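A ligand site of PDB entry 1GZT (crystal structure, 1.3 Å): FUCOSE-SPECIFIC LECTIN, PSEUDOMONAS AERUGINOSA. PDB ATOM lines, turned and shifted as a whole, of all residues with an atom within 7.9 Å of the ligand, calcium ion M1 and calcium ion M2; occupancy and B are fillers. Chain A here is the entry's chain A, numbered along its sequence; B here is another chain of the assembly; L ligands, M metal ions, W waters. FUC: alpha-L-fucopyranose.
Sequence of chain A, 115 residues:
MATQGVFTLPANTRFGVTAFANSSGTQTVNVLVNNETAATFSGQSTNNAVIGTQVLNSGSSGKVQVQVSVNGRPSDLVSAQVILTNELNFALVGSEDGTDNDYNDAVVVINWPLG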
ATOM      1  N   ALA A  21      12.722  13.835 -22.351  1.00  0.00           N
ATOM      2  CA  ALA A  21      11.531  13.826 -23.183  1.00  0.00           C
ATOM      3  C   ALA A  21      11.686  14.709 -24.414  1.00  0.00           C
ATOM      4  O   ALA A  21      12.250  15.821 -24.343  1.00  0.00           O
ATOM      5  CB  ALA A  21      10.315  14.267 -22.367  1.00  0.00           C
ATOM      6  N   ASN A  22      11.175  14.195 -25.534  1.00  0.00           N
ATOM      7  CA  ASN A  22      11.188  14.899 -26.819  1.00  0.00           C
ATOM      8  C   ASN A  22       9.964  14.542 -27.627  1.00  0.00           C
ATOM      9  O   ASN A  22      10.038  13.805 -28.598  1.00  0.00           O
ATOM     10  CB  ASN A  22      12.438  14.543 -27.660  1.00  0.00           C
ATOM     11  CG  ASN A  22      13.715  15.051 -27.068  1.00  0.00           C
ATOM     12  OD1 ASN A  22      14.057  16.238 -27.193  1.00  0.00           O
ATOM     13  ND2 ASN A  22      14.450  14.148 -26.422  1.00  0.00           N
ATOM     14  N   SER A  23       8.810  15.035 -27.193  1.00  0.00           N
ATOM     15  CA  SER A  23       7.548  14.687 -27.831  1.00  0.00           C
ATOM     16  C   SER A  23       6.449  15.633 -27.343  1.00  0.00           C
ATOM     17  O   SER A  23       6.525  16.220 -26.255  1.00  0.00           O
ATOM     18  CB  SER A  23       7.170  13.256 -27.464  1.00  0.00           C
ATOM     19  OG  SER A  23       5.859  12.951 -27.863  1.00  0.00           O
ATOM     20  N   SER A  24       5.388  15.755 -28.143  1.00  0.00           N
ATOM     21  CA  SER A  24       4.185  16.478 -27.693  1.00  0.00           C
ATOM     22  C   SER A  24       3.511  15.793 -26.510  1.00  0.00           C
ATOM     23  O   SER A  24       2.868  16.461 -25.706  1.00  0.00           O
ATOM     24  CB  SER A  24       3.163  16.561 -28.807  1.00  0.00           C
ATOM     25  OG  SER A  24       2.679  15.270 -29.130  1.00  0.00           O
ATOM     26  N   GLY A  25       3.673  14.481 -26.406  1.00  0.00           N
ATOM     27  CA  GLY A  25       2.976  13.737 -25.367  1.00  0.00           C
ATOM     28  C   GLY A  25       3.722  13.522 -24.074  1.00  0.00           C
ATOM     29  O   GLY A  25       4.955  13.451 -24.064  1.00  0.00           O
ATOM     30  N   GLN A  27       5.336  11.605 -21.273  1.00  0.00           N
ATOM     31  CA  GLN A  27       6.006  10.315 -21.168  1.00  0.00           C
ATOM     32  C   GLN A  27       5.942   9.809 -19.737  1.00  0.00           C
ATOM     33  O   GLN A  27       6.220  10.574 -18.818  1.00  0.00           O
ATOM     34  CB  GLN A  27       7.484  10.473 -21.559  1.00  0.00           C
ATOM     35  CG  GLN A  27       7.770  11.197 -22.871  1.00  0.00           C
ATOM     36  CD  GLN A  27       7.279  10.445 -24.087  1.00  0.00           C
ATOM     37  OE1 GLN A  27       6.453  10.999 -24.903  1.00  0.00           O
ATOM     38  NE2 GLN A  27       7.723   9.227 -24.245  1.00  0.00           N
ATOM     39  N   GLN A  44       6.644  16.146 -19.797  1.00  0.00           N
ATOM     40  CA  GLN A  44       6.446  16.487 -21.190  1.00  0.00           C
ATOM     41  C   GLN A  44       7.416  17.580 -21.595  1.00  0.00           C
ATOM     42  O   GLN A  44       7.551  18.575 -20.884  1.00  0.00           O
ATOM     43  CB  GLN A  44       4.987  16.927 -21.427  1.00  0.00           C
ATOM     44  CG  GLN A  44       4.629  17.147 -22.908  1.00  0.00           C
ATOM     45  CD  GLN A  44       5.133  18.493 -23.458  1.00  0.00           C
ATOM     46  OE1 GLN A  44       5.002  19.518 -22.788  1.00  0.00           O
ATOM     47  NE2 GLN A  44       5.680  18.494 -24.668  1.00  0.00           N
ATOM     48  N   SER A  45       8.115  17.366 -22.703  1.00  0.00           N
ATOM     49  CA  SER A  45       9.029  18.353 -23.246  1.00  0.00           C
ATOM     50  C   SER A  45       9.303  18.024 -24.705  1.00  0.00           C
ATOM     51  O   SER A  45       9.322  16.850 -25.074  1.00  0.00           O
ATOM     52  CB  SER A  45      10.360  18.302 -22.508  1.00  0.00           C
ATOM     53  OG  SER A  45      11.304  19.201 -23.045  1.00  0.00           O
ATOM     54  N   THR A  46       9.486  19.046 -25.524  1.00  0.00           N
ATOM     55  CA  THR A  46      10.033  18.859 -26.852  1.00  0.00           C
ATOM     56  C   THR A  46      11.449  19.425 -26.926  1.00  0.00           C
ATOM     57  O   THR A  46      11.979  19.620 -28.029  1.00  0.00           O
ATOM     58  CB  THR A  46       9.180  19.546 -27.924  1.00  0.00           C
ATOM     59  OG1 THR A  46       8.826  20.860 -27.505  1.00  0.00           O
ATOM     60  CG2 THR A  46       7.873  18.785 -28.158  1.00  0.00           C
ATOM     61  N   VAL A  70       2.899   6.269 -23.296  1.00  0.00           N
ATOM     62  CA  VAL A  70       2.444   7.585 -23.701  1.00  0.00           C
ATOM     63  C   VAL A  70       1.004   7.468 -24.178  1.00  0.00           C
ATOM     64  O   VAL A  70       0.719   6.586 -24.988  1.00  0.00           O
ATOM     65  CB  VAL A  70       3.305   8.159 -24.866  1.00  0.00           C
ATOM     66  CG1 VAL A  70       2.896   9.595 -25.172  1.00  0.00           C
ATOM     67  CG2 VAL A  70       4.778   8.102 -24.521  1.00  0.00           C
ATOM     68  N   SER A  95      12.705   5.427 -27.531  1.00  0.00           N
ATOM     69  CA  SER A  95      11.313   4.983 -27.602  1.00  0.00           C
ATOM     70  C   SER A  95      10.547   5.859 -28.575  1.00  0.00           C
ATOM     71  O   SER A  95      10.864   7.036 -28.743  1.00  0.00           O
ATOM     72  CB  SER A  95      10.693   5.012 -26.226  1.00  0.00           C
ATOM     73  OG  SER A  95      10.600   6.324 -25.719  1.00  0.00           O
ATOM     74  N   GLU A  96       9.557   5.241 -29.217  1.00  0.00           N
ATOM     75  CA  GLU A  96       8.736   5.887 -30.227  1.00  0.00           C
ATOM     76  C   GLU A  96       7.264   5.779 -29.852  1.00  0.00           C
ATOM     77  O   GLU A  96       6.736   4.694 -29.697  1.00  0.00           O
ATOM     78  CB  GLU A  96       9.009   5.265 -31.609  1.00  0.00           C
ATOM     79  CG  GLU A  96       8.170   5.858 -32.722  1.00  0.00           C
ATOM     80  CD  GLU A  96       8.292   7.364 -32.780  1.00  0.00           C
ATOM     81  OE1 GLU A  96       9.437   7.872 -32.811  1.00  0.00           O
ATOM     82  OE2 GLU A  96       7.275   8.095 -32.801  1.00  0.00           O
ATOM     83  N   ASP A  97       6.638   6.944 -29.709  1.00  0.00           N
ATOM     84  CA  ASP A  97       5.252   7.026 -29.287  1.00  0.00           C
ATOM     85  C   ASP A  97       4.297   7.344 -30.437  1.00  0.00           C
ATOM     86  O   ASP A  97       3.075   7.430 -30.211  1.00  0.00           O
ATOM     87  CB  ASP A  97       5.113   8.060 -28.153  1.00  0.00           C
ATOM     88  CG  ASP A  97       5.323   9.501 -28.602  1.00  0.00           C
ATOM     89  OD1 ASP A  97       5.160   9.841 -29.799  1.00  0.00           O
ATOM     90  OD2 ASP A  97       5.566  10.397 -27.767  1.00  0.00           O
ATOM     91  N   GLY A  98       4.825   7.485 -31.655  1.00  0.00           N
ATOM     92  CA  GLY A  98       4.043   7.930 -32.791  1.00  0.00           C
ATOM     93  C   GLY A  98       4.448   7.295 -34.096  1.00  0.00           C
ATOM     94  O   GLY A  98       4.717   6.098 -34.146  1.00  0.00           O
ATOM     95  N   THR A  99       4.519   8.126 -35.135  1.00  0.00           N
ATOM     96  CA  THR A  99       4.728   7.641 -36.496  1.00  0.00           C
ATOM     97  C   THR A  99       5.992   8.158 -37.182  1.00  0.00           C
ATOM     98  O   THR A  99       6.327   7.665 -38.251  1.00  0.00           O
ATOM     99  CB  THR A  99       3.523   8.031 -37.383  1.00  0.00           C
ATOM    100  OG1 THR A  99       3.376   9.454 -37.414  1.00  0.00           O
ATOM    101  CG2 THR A  99       2.189   7.472 -36.825  1.00  0.00           C
ATOM    102  N   ASP A 100       6.684   9.144 -36.606  1.00  0.00           N
ATOM    103  CA  ASP A 100       7.857   9.730 -37.267  1.00  0.00           C
ATOM    104  C   ASP A 100       9.141   8.925 -37.110  1.00  0.00           C
ATOM    105  O   ASP A 100      10.105   9.191 -37.799  1.00  0.00           O
ATOM    106  CB  ASP A 100       8.091  11.190 -36.883  1.00  0.00           C
ATOM    107  CG  ASP A 100       8.538  11.373 -35.459  1.00  0.00           C
ATOM    108  OD1 ASP A 100       8.422  10.414 -34.662  1.00  0.00           O
ATOM    109  OD2 ASP A 100       8.936  12.499 -35.098  1.00  0.00           O
ATOM    110  N   ASN A 101       9.134   7.961 -36.200  1.00  0.00           N
ATOM    111  CA  ASN A 101      10.286   7.094 -36.002  1.00  0.00           C
ATOM    112  C   ASN A 101      11.591   7.832 -35.685  1.00  0.00           C
ATOM    113  O   ASN A 101      12.673   7.433 -36.106  1.00  0.00           O
ATOM    114  CB  ASN A 101      10.439   6.156 -37.197  1.00  0.00           C
ATOM    115  CG  ASN A 101       9.284   5.208 -37.299  1.00  0.00           C
ATOM    116  OD1 ASN A 101       8.643   4.875 -36.302  1.00  0.00           O
ATOM    117  ND2 ASN A 101       8.995   4.761 -38.519  1.00  0.00           N
ATOM    118  N   ASP A 102      11.493   8.909 -34.909  1.00  0.00           N
ATOM    119  CA  ASP A 102      12.690   9.546 -34.372  1.00  0.00           C
ATOM    120  C   ASP A 102      13.237   8.806 -33.133  1.00  0.00           C
ATOM    121  O   ASP A 102      14.442   8.928 -32.844  1.00  0.00           O
ATOM    122  CB  ASP A 102      12.544  11.056 -34.198  1.00  0.00           C
ATOM    123  CG  ASP A 102      11.543  11.503 -33.143  1.00  0.00           C
ATOM    124  OD1 ASP A 102      10.819  10.637 -32.575  1.00  0.00           O
ATOM    125  OD2 ASP A 102      11.460  12.715 -32.857  1.00  0.00           O
ATOM    126  N   TYR A 103      12.395   8.012 -32.464  1.00  0.00           N
ATOM    127  CA  TYR A 103      12.805   7.192 -31.330  1.00  0.00           C
ATOM    128  C   TYR A 103      13.443   7.964 -30.163  1.00  0.00           C
ATOM    129  O   TYR A 103      14.152   7.378 -29.326  1.00  0.00           O
ATOM    130  CB  TYR A 103      13.679   6.011 -31.795  1.00  0.00           C
ATOM    131  CG  TYR A 103      12.806   4.868 -32.328  1.00  0.00           C
ATOM    132  CD1 TYR A 103      12.310   3.911 -31.455  1.00  0.00           C
ATOM    133  CD2 TYR A 103      12.365   4.869 -33.627  1.00  0.00           C
ATOM    134  CE1 TYR A 103      11.478   2.927 -31.889  1.00  0.00           C
ATOM    135  CE2 TYR A 103      11.502   3.874 -34.087  1.00  0.00           C
ATOM    136  CZ  TYR A 103      11.069   2.927 -33.197  1.00  0.00           C
ATOM    137  OH  TYR A 103      10.190   1.949 -33.650  1.00  0.00           O
ATOM    138  N   ASN A 104      13.138   9.254 -30.043  1.00  0.00           N
ATOM    139  CA  ASN A 104      13.675  10.070 -28.957  1.00  0.00           C
ATOM    140  C   ASN A 104      12.611  10.547 -27.991  1.00  0.00           C
ATOM    141  O   ASN A 104      12.860  11.398 -27.162  1.00  0.00           O
ATOM    142  CB  ASN A 104      14.414  11.275 -29.543  1.00  0.00           C
ATOM    143  CG  ASN A 104      13.465  12.317 -30.130  1.00  0.00           C
ATOM    144  OD1 ASN A 104      12.247  12.116 -30.143  1.00  0.00           O
ATOM    145  ND2 ASN A 104      14.010  13.429 -30.609  1.00  0.00           N
ATOM    146  N   ASP A 105      11.410   9.994 -28.115  1.00  0.00           N
ATOM    147  CA  ASP A 105      10.250  10.597 -27.441  1.00  0.00           C
ATOM    148  C   ASP A 105      10.434  10.547 -25.938  1.00  0.00           C
ATOM    149  O   ASP A 105      10.159  11.500 -25.213  1.00  0.00           O
ATOM    150  CB  ASP A 105       8.957   9.934 -27.927  1.00  0.00           C
ATOM    151  CG  ASP A 105       8.768  10.118 -29.411  1.00  0.00           C
ATOM    152  OD1 ASP A 105       9.160  11.189 -29.932  1.00  0.00           O
ATOM    153  OD2 ASP A 105       8.244   9.260 -30.147  1.00  0.00           O
ATOM    154  N   ALA A 106      10.907   9.392 -25.458  1.00  0.00           N
ATOM    155  CA  ALA A 106      11.569   9.295 -24.155  1.00  0.00           C
ATOM    156  C   ALA A 106      12.922   8.624 -24.443  1.00  0.00           C
ATOM    157  O   ALA A 106      12.961   7.583 -25.127  1.00  0.00           O
ATOM    158  CB  ALA A 106      10.798   8.497 -23.126  1.00  0.00           C
ATOM    159  N   GLU B  87      19.051   5.885 -36.573  1.00  0.00           N
ATOM    160  CA  GLU B  87      18.535   7.232 -36.420  1.00  0.00           C
ATOM    161  C   GLU B  87      18.782   7.918 -35.075  1.00  0.00           C
ATOM    162  O   GLU B  87      18.835   9.132 -35.020  1.00  0.00           O
ATOM    163  CB  GLU B  87      17.026   7.222 -36.699  1.00  0.00           C
ATOM    164  CG  GLU B  87      16.415   8.609 -36.839  1.00  0.00           C
ATOM    165  CD  GLU B  87      16.027   9.185 -35.502  1.00  0.00           C
ATOM    166  OE1 GLU B  87      15.986   8.401 -34.537  1.00  0.00           O
ATOM    167  OE2 GLU B  87      15.759  10.405 -35.397  1.00  0.00           O
ATOM    168  N   PRO B 113      18.744  13.076 -32.538  1.00  0.00           N
ATOM    169  CA  PRO B 113      18.074  14.373 -32.583  1.00  0.00           C
ATOM    170  C   PRO B 113      17.167  14.619 -31.406  1.00  0.00           C
ATOM    171  O   PRO B 113      16.825  13.700 -30.658  1.00  0.00           O
ATOM    172  CB  PRO B 113      17.168  14.238 -33.820  1.00  0.00           C
ATOM    173  CG  PRO B 113      16.892  12.779 -33.940  1.00  0.00           C
ATOM    174  CD  PRO B 113      18.142  12.111 -33.466  1.00  0.00           C
ATOM    175  N   LEU B 114      16.781  15.879 -31.261  1.00  0.00           N
ATOM    176  CA  LEU B 114      15.843  16.291 -30.232  1.00  0.00           C
ATOM    177  C   LEU B 114      14.514  16.622 -30.891  1.00  0.00           C
ATOM    178  O   LEU B 114      14.387  16.573 -32.111  1.00  0.00           O
ATOM    179  CB  LEU B 114      16.360  17.560 -29.548  1.00  0.00           C
ATOM    180  CG  LEU B 114      17.749  17.453 -28.927  1.00  0.00           C
ATOM    181  CD1 LEU B 114      18.030  18.691 -28.110  1.00  0.00           C
ATOM    182  CD2 LEU B 114      17.872  16.238 -28.060  1.00  0.00           C
ATOM    183  N   GLY B 115      13.534  16.957 -30.072  1.00  0.00           N
ATOM    184  CA  GLY B 115      12.250  17.415 -30.573  1.00  0.00           C
ATOM    185  C   GLY B 115      11.186  16.361 -30.820  1.00  0.00           C
ATOM    186  O   GLY B 115      11.507  15.157 -30.951  1.00  0.00           O
ATOM    187  OXT GLY B 115      10.019  16.779 -30.918  1.00  0.00           O
HETATM  188  C1  FUC L   1       5.287  13.458 -31.281  1.00  0.00           C
HETATM  189  C2  FUC L   1       6.528  12.614 -31.351  1.00  0.00           C
HETATM  190  C3  FUC L   1       7.329  13.258 -32.471  1.00  0.00           C
HETATM  191  C4  FUC L   1       7.561  14.708 -32.160  1.00  0.00           C
HETATM  192  C5  FUC L   1       6.236  15.402 -31.864  1.00  0.00           C
HETATM  193  C6  FUC L   1       6.437  16.846 -31.466  1.00  0.00           C
HETATM  194  O1  FUC L   1       4.411  13.233 -32.320  1.00  0.00           O
HETATM  195  O2  FUC L   1       6.335  11.236 -31.686  1.00  0.00           O
HETATM  196  O3  FUC L   1       8.576  12.570 -32.585  1.00  0.00           O
HETATM  197  O4  FUC L   1       8.469  14.766 -31.056  1.00  0.00           O
HETATM  198  O5  FUC L   1       5.519  14.708 -30.848  1.00  0.00           O
HETATM  199 CA    CA M   1       8.520  10.114 -32.321  1.00  0.00          CA
HETATM  200 CA    CA M   2      10.258  13.076 -30.835  1.00  0.00          CA
HETATM  201  O   HOH W   1       5.048  10.977 -34.466  1.00  0.00           O
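The side-chain amide oxygen (OD1) of Asn 104 binds calcium ion M2 (2.3 Å).
Calcium ion M2 is bound by the side-chain carboxylate (OD1) of Asp 105.
Calcium ion M2 is bound by O of Asn 22 (2.4 Å).
OD2 of Asp 102 binds calcium ion M2, 2.4 Å away.
Calcium ion M2 is bound by the chain-end carboxylate (O) of Gly 115 of chain B (2.4 Å).
O4 of the ligand is bound to calcium ion M2, at 2.5 Å.
O3 of the ligand is bound to calcium ion M2 (2.5 Å).
Slightly farther from calcium ion M2 lies the side-chain carboxylate (OD1) of Asp 102 (3.0 Å).
OD2 of Asp 105 binds calcium ion M1 (2.4 Å).
Calcium ion M1 is bound by OD1 of Asp 100 (2.4 Å).
OD1 of Asp 102 is bound to calcium ion M1 (2.4 Å).
OE2 of Glu 96 binds calcium ion M1, 2.4 Å away.
OE1 of Glu 96 binds calcium ion M1 (2.5 Å).
Calcium ion M1 is bound by O3 of the ligand (2.5 Å).
O2 of the ligand binds calcium ion M1.
OD1 of Asp 105 binds calcium ion M1.
The side-chain carboxylate (OE1) of Glu 96 lies close to the backbone NH (N) of Tyr 103, 3.0 Å away.
The backbone carbonyl oxygen (O) of Ser 23 lies within hydrogen-bond range of the side-chain amide nitrogen (NE2) of Gln 44.
The side-chain carboxylate (OD2) of Asp 105 sits close to the backbone NH (N) of Asp 97, at 2.9 Å.
ND2 of Asn 104 is in hydrogen-bond range of O of Pro 113 of chain B.
The backbone NH (N) of Asp 105 sits at hydrogen-bond distance from the backbone carbonyl oxygen (O) of Ser 95, 3.1 Å away.
N of Asn 101 sits close to OE1 of Glu 96 (3.4 Å).
OG of Ser 23 is in hydrogen-bond range of OD2 of Asp 97 (2.6 Å).
The side-chain hydroxyl (OG) of Ser 23 lies within hydrogen-bond range of the backbone NH (N) of Gly 25, 3.0 Å away.
The backbone NH (N) of Ser 24 lies within hydrogen-bond range of an oxygen (O5) of the ligand (2.9 Å).
The side-chain hydroxyl (OG) of Ser 23 sits at hydrogen-bond distance from an oxygen (O5) of the ligand.
The side-chain carboxylate (OD1) of Asp 97 sits close to an oxygen (O2) of the ligand, at 2.6 Å.
The side-chain hydroxyl (OG) of Ser 24 lies within hydrogen-bond range of an oxygen (O5) of the ligand (3.4 Å).
Within 4 Å of the ligand: Asn 22, Ser 23, Ser 24, Glu 96, Asp 97, Asp 100, Asp 102, Asp 105 and Gly 115 of chain B.
The nearest printed residue that does not touch the ligand is Gly 98 (4.04 Å).
Of the 26 residues printed, 5 come within 4 Å of calcium ion M2.
Water W1 lies within hydrogen-bond range of N of Thr 99 (3.0 Å), O1 of the ligand (3.2 Å) and N of Asp 100 (3.3 Å).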
